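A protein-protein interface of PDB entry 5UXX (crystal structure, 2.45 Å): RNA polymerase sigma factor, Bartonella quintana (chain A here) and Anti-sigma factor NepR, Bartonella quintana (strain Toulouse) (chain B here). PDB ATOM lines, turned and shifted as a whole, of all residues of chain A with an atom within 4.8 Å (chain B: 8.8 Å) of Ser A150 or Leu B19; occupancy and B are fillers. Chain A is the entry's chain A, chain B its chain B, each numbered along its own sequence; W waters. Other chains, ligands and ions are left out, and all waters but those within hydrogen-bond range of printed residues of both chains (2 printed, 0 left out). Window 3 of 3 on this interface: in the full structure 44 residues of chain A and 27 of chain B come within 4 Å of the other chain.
Among the printed residues, merely in contact across the chains: Tyr A131 with Leu B19 (3.5 Å), Lys A146 with Leu B19 (3.6 Å), Ser A150 with Leu B19 (3.8 Å), Arg A153 with Ser B24 (3.4 Å) and Arg A153 with Ile B26 (3.7 Å).
Of the printed residues of chain B, Tyr A131 touches Leu B19 (3.5 Å). Printed residues of chain B within 4 Å of Lys A146: Leu B19. No residue of chain B comes within 4 Å of Val A149. Of chain B, only Leu B19 comes within 4 Å of Ser A150. Of the printed residues of chain B, Arg A153 touches Leu B19 (3.2 Å), Leu B20 (3.5 Å), Ser B24 (3.4 Å) and Ile B26 (3.7 Å). Leu B19 touches four residues of chain A. Of the printed residues of chain A, Leu B20 touches Arg A153. Of the printed residues of chain A, Ile B26 touches Arg A153 (3.7 Å). The nearest residue of chain A that does not touch Leu B19 is Val A149 (4.4 Å). The nearest printed residue of chain B that does not touch Lys A146 is Asp B17 (7.0 Å).
The backbone carbonyl oxygen of Lys A146 lies within hydrogen-bond range of the side-chain hydroxyl of Ser A150 (3.2 Å). The side-chain amide nitrogen (ND2) of Asn A154 sits at hydrogen-bond distance from the backbone carbonyl oxygen (O) of Ser A150 (3.3 Å). O of Leu B20 lies within hydrogen-bond range of OG of Ser B24, 3.1 Å away. O of Gly B21 lies within hydrogen-bond range of OG of Ser B24, 2.7 Å away. The side-chain hydroxyl (OG) of Ser B24 sits at hydrogen-bond distance from the backbone NH (N) of Ala B27 (3.3 Å).
Water W1 bridges OH of Tyr A131 (2.8 Å) and O of Asp B17 (3.5 Å). Water W2 bridges the backbone carbonyl oxygen (O) of Leu B19 and the side-chain hydroxyl (OG) of Ser A150.
Hydrophobic or aromatic side chains of chain A that line the printed part of chain B: Tyr A131. Of the 12 printed residues of chain B, 4 touch a printed residue of chain A. Among the printed residues, 7 pairs touch across the chains. Among the printed residues, no Asp or Glu carboxylate lies within 4 Å of a Lys or Arg side-chain nitrogen of the other chain.
The backbone carbonyl oxygen (O) of Leu B19 lies within hydrogen-bond range of the guanidinium group (NH1) of Arg A153, 3.2 Å away. The guanidinium group (NE) of Arg A153 lies within hydrogen-bond range of the backbone carbonyl oxygen (O) of Leu B20 (3.5 Å).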
ATOM      1  N   TYR A 131     -38.611   2.215  -0.442  1.00  0.00           N
ATOM      2  CA  TYR A 131     -37.949   3.258   0.336  1.00  0.00           C
ATOM      3  C   TYR A 131     -38.982   4.178   0.974  1.00  0.00           C
ATOM      4  O   TYR A 131     -38.819   4.617   2.113  1.00  0.00           O
ATOM      5  CB  TYR A 131     -36.989   4.068  -0.539  1.00  0.00           C
ATOM      6  CG  TYR A 131     -35.796   3.279  -1.031  1.00  0.00           C
ATOM      7  CD1 TYR A 131     -34.848   2.791  -0.141  1.00  0.00           C
ATOM      8  CD2 TYR A 131     -35.613   3.032  -2.385  1.00  0.00           C
ATOM      9  CE1 TYR A 131     -33.756   2.071  -0.584  1.00  0.00           C
ATOM     10  CE2 TYR A 131     -34.522   2.314  -2.838  1.00  0.00           C
ATOM     11  CZ  TYR A 131     -33.598   1.836  -1.934  1.00  0.00           C
ATOM     12  OH  TYR A 131     -32.510   1.120  -2.379  1.00  0.00           O
ATOM     13  N   LYS A 146     -32.080   5.515   2.730  1.00  0.00           N
ATOM     14  CA  LYS A 146     -31.119   5.154   1.694  1.00  0.00           C
ATOM     15  C   LYS A 146     -29.683   5.159   2.211  1.00  0.00           C
ATOM     16  O   LYS A 146     -28.908   4.248   1.916  1.00  0.00           O
ATOM     17  CB  LYS A 146     -31.253   6.102   0.502  1.00  0.00           C
ATOM     18  CG  LYS A 146     -32.499   5.853  -0.331  1.00  0.00           C
ATOM     19  CD  LYS A 146     -32.620   6.841  -1.478  1.00  0.00           C
ATOM     20  CE  LYS A 146     -33.826   6.519  -2.344  1.00  0.00           C
ATOM     21  NZ  LYS A 146     -34.033   7.537  -3.410  1.00  0.00           N
ATOM     22  N   SER A 147     -29.330   6.182   2.983  1.00  0.00           N
ATOM     23  CA  SER A 147     -27.990   6.273   3.553  1.00  0.00           C
ATOM     24  C   SER A 147     -27.777   5.185   4.602  1.00  0.00           C
ATOM     25  O   SER A 147     -26.690   4.618   4.710  1.00  0.00           O
ATOM     26  CB  SER A 147     -27.753   7.654   4.166  1.00  0.00           C
ATOM     27  OG  SER A 147     -28.544   7.841   5.325  1.00  0.00           O
ATOM     28  N   ARG A 148     -28.825   4.895   5.368  1.00  0.00           N
ATOM     29  CA  ARG A 148     -28.773   3.835   6.369  1.00  0.00           C
ATOM     30  C   ARG A 148     -28.611   2.469   5.710  1.00  0.00           C
ATOM     31  O   ARG A 148     -27.893   1.610   6.217  1.00  0.00           O
ATOM     32  CB  ARG A 148     -30.026   3.859   7.249  1.00  0.00           C
ATOM     33  CG  ARG A 148     -30.044   5.001   8.252  1.00  0.00           C
ATOM     34  CD  ARG A 148     -31.344   5.064   9.034  1.00  0.00           C
ATOM     35  NE  ARG A 148     -31.329   6.157  10.001  1.00  0.00           N
ATOM     36  CZ  ARG A 148     -32.360   6.496  10.768  1.00  0.00           C
ATOM     37  NH1 ARG A 148     -33.501   5.826  10.684  1.00  0.00           N
ATOM     38  NH2 ARG A 148     -32.251   7.506  11.619  1.00  0.00           N
ATOM     39  N   VAL A 149     -29.285   2.273   4.580  1.00  0.00           N
ATOM     40  CA  VAL A 149     -29.183   1.026   3.832  1.00  0.00           C
ATOM     41  C   VAL A 149     -27.770   0.843   3.279  1.00  0.00           C
ATOM     42  O   VAL A 149     -27.195  -0.242   3.368  1.00  0.00           O
ATOM     43  CB  VAL A 149     -30.205   0.976   2.675  1.00  0.00           C
ATOM     44  CG1 VAL A 149     -29.833  -0.099   1.662  1.00  0.00           C
ATOM     45  CG2 VAL A 149     -31.608   0.741   3.218  1.00  0.00           C
ATOM     46  N   SER A 150     -27.212   1.915   2.725  1.00  0.00           N
ATOM     47  CA  SER A 150     -25.872   1.875   2.147  1.00  0.00           C
ATOM     48  C   SER A 150     -24.803   1.579   3.195  1.00  0.00           C
ATOM     49  O   SER A 150     -23.914   0.758   2.965  1.00  0.00           O
ATOM     50  CB  SER A 150     -25.556   3.196   1.442  1.00  0.00           C
ATOM     51  OG  SER A 150     -26.332   3.346   0.266  1.00  0.00           O
ATOM     52  N   ARG A 151     -24.886   2.251   4.339  1.00  0.00           N
ATOM     53  CA  ARG A 151     -23.923   2.036   5.414  1.00  0.00           C
ATOM     54  C   ARG A 151     -24.054   0.633   6.003  1.00  0.00           C
ATOM     55  O   ARG A 151     -23.052  -0.025   6.288  1.00  0.00           O
ATOM     56  CB  ARG A 151     -24.083   3.092   6.515  1.00  0.00           C
ATOM     57  CG  ARG A 151     -23.673   4.494   6.081  1.00  0.00           C
ATOM     58  CD  ARG A 151     -23.821   5.527   7.195  1.00  0.00           C
ATOM     59  NE  ARG A 151     -25.204   5.722   7.623  1.00  0.00           N
ATOM     60  CZ  ARG A 151     -25.712   5.239   8.753  1.00  0.00           C
ATOM     61  NH1 ARG A 151     -26.978   5.468   9.065  1.00  0.00           N
ATOM     62  NH2 ARG A 151     -24.950   4.536   9.577  1.00  0.00           N
ATOM     63  N   ALA A 152     -25.291   0.178   6.179  1.00  0.00           N
ATOM     64  CA  ALA A 152     -25.545  -1.156   6.714  1.00  0.00           C
ATOM     65  C   ALA A 152     -25.046  -2.237   5.764  1.00  0.00           C
ATOM     66  O   ALA A 152     -24.476  -3.239   6.195  1.00  0.00           O
ATOM     67  CB  ALA A 152     -27.029  -1.344   6.993  1.00  0.00           C
ATOM     68  N   ARG A 153     -25.267  -2.030   4.470  1.00  0.00           N
ATOM     69  CA  ARG A 153     -24.854  -2.998   3.463  1.00  0.00           C
ATOM     70  C   ARG A 153     -23.334  -3.141   3.432  1.00  0.00           C
ATOM     71  O   ARG A 153     -22.814  -4.255   3.425  1.00  0.00           O
ATOM     72  CB  ARG A 153     -25.378  -2.596   2.082  1.00  0.00           C
ATOM     73  CG  ARG A 153     -25.091  -3.619   0.994  1.00  0.00           C
ATOM     74  CD  ARG A 153     -24.808  -2.954  -0.343  1.00  0.00           C
ATOM     75  NE  ARG A 153     -24.252  -3.899  -1.308  1.00  0.00           N
ATOM     76  CZ  ARG A 153     -23.979  -3.601  -2.574  1.00  0.00           C
ATOM     77  NH1 ARG A 153     -24.212  -2.380  -3.035  1.00  0.00           N
ATOM     78  NH2 ARG A 153     -23.473  -4.525  -3.380  1.00  0.00           N
ATOM     79  N   ASN A 154     -22.630  -2.013   3.428  1.00  0.00           N
ATOM     80  CA  ASN A 154     -21.171  -2.025   3.376  1.00  0.00           C
ATOM     81  C   ASN A 154     -20.545  -2.633   4.628  1.00  0.00           C
ATOM     82  O   ASN A 154     -19.510  -3.293   4.553  1.00  0.00           O
ATOM     83  CB  ASN A 154     -20.632  -0.608   3.173  1.00  0.00           C
ATOM     84  CG  ASN A 154     -20.894  -0.077   1.778  1.00  0.00           C
ATOM     85  OD1 ASN A 154     -21.102  -0.845   0.838  1.00  0.00           O
ATOM     86  ND2 ASN A 154     -20.882   1.243   1.635  1.00  0.00           N
ATOM     87  N   PHE B  15     -23.604   1.230 -11.955  1.00  0.00           N
ATOM     88  CA  PHE B  15     -24.959   1.249 -11.418  1.00  0.00           C
ATOM     89  C   PHE B  15     -24.953   1.655  -9.947  1.00  0.00           C
ATOM     90  O   PHE B  15     -25.285   0.857  -9.070  1.00  0.00           O
ATOM     91  CB  PHE B  15     -25.623  -0.121 -11.586  1.00  0.00           C
ATOM     92  CG  PHE B  15     -25.503  -0.687 -12.973  1.00  0.00           C
ATOM     93  CD1 PHE B  15     -26.128  -0.071 -14.046  1.00  0.00           C
ATOM     94  CD2 PHE B  15     -24.768  -1.839 -13.204  1.00  0.00           C
ATOM     95  CE1 PHE B  15     -26.019  -0.593 -15.323  1.00  0.00           C
ATOM     96  CE2 PHE B  15     -24.655  -2.366 -14.478  1.00  0.00           C
ATOM     97  CZ  PHE B  15     -25.283  -1.741 -15.539  1.00  0.00           C
ATOM     98  N   GLY B  16     -24.574   2.902  -9.686  1.00  0.00           N
ATOM     99  CA  GLY B  16     -24.457   3.401  -8.327  1.00  0.00           C
ATOM    100  C   GLY B  16     -25.786   3.611  -7.629  1.00  0.00           C
ATOM    101  O   GLY B  16     -25.854   3.608  -6.400  1.00  0.00           O
ATOM    102  N   ASP B  17     -26.845   3.793  -8.410  1.00  0.00           N
ATOM    103  CA  ASP B  17     -28.177   4.011  -7.856  1.00  0.00           C
ATOM    104  C   ASP B  17     -28.764   2.721  -7.288  1.00  0.00           C
ATOM    105  O   ASP B  17     -29.761   2.748  -6.565  1.00  0.00           O
ATOM    106  CB  ASP B  17     -29.111   4.594  -8.919  1.00  0.00           C
ATOM    107  CG  ASP B  17     -28.615   5.921  -9.462  1.00  0.00           C
ATOM    108  OD1 ASP B  17     -27.831   6.596  -8.762  1.00  0.00           O
ATOM    109  OD2 ASP B  17     -29.009   6.290 -10.590  1.00  0.00           O
ATOM    110  N   ASP B  18     -28.143   1.593  -7.622  1.00  0.00           N
ATOM    111  CA  ASP B  18     -28.559   0.300  -7.093  1.00  0.00           C
ATOM    112  C   ASP B  18     -27.950   0.090  -5.709  1.00  0.00           C
ATOM    113  O   ASP B  18     -26.863  -0.471  -5.577  1.00  0.00           O
ATOM    114  CB  ASP B  18     -28.147  -0.825  -8.045  1.00  0.00           C
ATOM    115  CG  ASP B  18     -28.623  -2.190  -7.584  1.00  0.00           C
ATOM    116  OD1 ASP B  18     -29.490  -2.255  -6.689  1.00  0.00           O
ATOM    117  OD2 ASP B  18     -28.129  -3.201  -8.126  1.00  0.00           O
ATOM    118  N   LEU B  19     -28.663   0.542  -4.683  1.00  0.00           N
ATOM    119  CA  LEU B  19     -28.141   0.546  -3.320  1.00  0.00           C
ATOM    120  C   LEU B  19     -27.984  -0.855  -2.740  1.00  0.00           C
ATOM    121  O   LEU B  19     -26.982  -1.159  -2.094  1.00  0.00           O
ATOM    122  CB  LEU B  19     -29.048   1.380  -2.414  1.00  0.00           C
ATOM    123  CG  LEU B  19     -29.286   2.821  -2.869  1.00  0.00           C
ATOM    124  CD1 LEU B  19     -30.123   3.568  -1.848  1.00  0.00           C
ATOM    125  CD2 LEU B  19     -27.964   3.534  -3.110  1.00  0.00           C
ATOM    126  N   LEU B  20     -28.978  -1.704  -2.973  1.00  0.00           N
ATOM    127  CA  LEU B  20     -28.961  -3.056  -2.433  1.00  0.00           C
ATOM    128  C   LEU B  20     -27.978  -3.951  -3.183  1.00  0.00           C
ATOM    129  O   LEU B  20     -27.348  -4.827  -2.590  1.00  0.00           O
ATOM    130  CB  LEU B  20     -30.364  -3.662  -2.481  1.00  0.00           C
ATOM    131  CG  LEU B  20     -30.786  -4.509  -1.280  1.00  0.00           C
ATOM    132  CD1 LEU B  20     -30.416  -3.818   0.024  1.00  0.00           C
ATOM    133  CD2 LEU B  20     -32.279  -4.792  -1.337  1.00  0.00           C
ATOM    134  N   GLY B  21     -27.845  -3.726  -4.486  1.00  0.00           N
ATOM    135  CA  GLY B  21     -27.003  -4.571  -5.310  1.00  0.00           C
ATOM    136  C   GLY B  21     -27.733  -5.822  -5.758  1.00  0.00           C
ATOM    137  O   GLY B  21     -27.691  -6.849  -5.080  1.00  0.00           O
ATOM    138  N   VAL B  22     -28.407  -5.733  -6.902  1.00  0.00           N
ATOM    139  CA  VAL B  22     -29.277  -6.806  -7.374  1.00  0.00           C
ATOM    140  C   VAL B  22     -28.509  -8.101  -7.645  1.00  0.00           C
ATOM    141  O   VAL B  22     -29.086  -9.186  -7.620  1.00  0.00           O
ATOM    142  CB  VAL B  22     -30.035  -6.392  -8.650  1.00  0.00           C
ATOM    143  CG1 VAL B  22     -30.990  -5.246  -8.348  1.00  0.00           C
ATOM    144  CG2 VAL B  22     -29.062  -6.006  -9.754  1.00  0.00           C
ATOM    145  N   SER B  24     -25.605  -8.783  -5.847  1.00  0.00           N
ATOM    146  CA  SER B  24     -24.678  -8.886  -4.727  1.00  0.00           C
ATOM    147  C   SER B  24     -25.022 -10.095  -3.864  1.00  0.00           C
ATOM    148  O   SER B  24     -26.173 -10.527  -3.823  1.00  0.00           O
ATOM    149  CB  SER B  24     -24.706  -7.609  -3.883  1.00  0.00           C
ATOM    150  OG  SER B  24     -25.913  -7.509  -3.144  1.00  0.00           O
ATOM    151  N   ILE B  26     -24.787 -10.150  -0.576  1.00  0.00           N
ATOM    152  CA  ILE B  26     -25.414  -9.688   0.661  1.00  0.00           C
ATOM    153  C   ILE B  26     -26.929  -9.534   0.494  1.00  0.00           C
ATOM    154  O   ILE B  26     -27.691  -9.762   1.435  1.00  0.00           O
ATOM    155  CB  ILE B  26     -24.796  -8.353   1.152  1.00  0.00           C
ATOM    156  CG1 ILE B  26     -25.366  -7.966   2.519  1.00  0.00           C
ATOM    157  CG2 ILE B  26     -25.007  -7.236   0.137  1.00  0.00           C
ATOM    158  CD1 ILE B  26     -25.024  -8.947   3.617  1.00  0.00           C
ATOM    159  N   ALA B  27     -27.363  -9.166  -0.708  1.00  0.00           N
ATOM    160  CA  ALA B  27     -28.786  -9.061  -1.002  1.00  0.00           C
ATOM    161  C   ALA B  27     -29.432 -10.439  -0.956  1.00  0.00           C
ATOM    162  O   ALA B  27     -30.572 -10.592  -0.521  1.00  0.00           O
ATOM    163  CB  ALA B  27     -29.008  -8.413  -2.360  1.00  0.00           C
ATOM    164  N   LEU B  30     -29.598 -11.745   2.776  1.00  0.00           N
ATOM    165  CA  LEU B  30     -30.691 -11.103   3.498  1.00  0.00           C
ATOM    166  C   LEU B  30     -32.009 -11.826   3.238  1.00  0.00           C
ATOM    167  O   LEU B  30     -32.795 -12.049   4.159  1.00  0.00           O
ATOM    168  CB  LEU B  30     -30.805  -9.628   3.106  1.00  0.00           C
ATOM    169  CG  LEU B  30     -29.765  -8.696   3.734  1.00  0.00           C
ATOM    170  CD1 LEU B  30     -29.620  -7.418   2.922  1.00  0.00           C
ATOM    171  CD2 LEU B  30     -30.132  -8.379   5.176  1.00  0.00           C
HETATM  172  O   HOH W   1     -32.342   0.880  -5.163  1.00  0.00           O
HETATM  173  O   HOH W   2     -25.020   0.683  -1.040  1.00  0.00           O
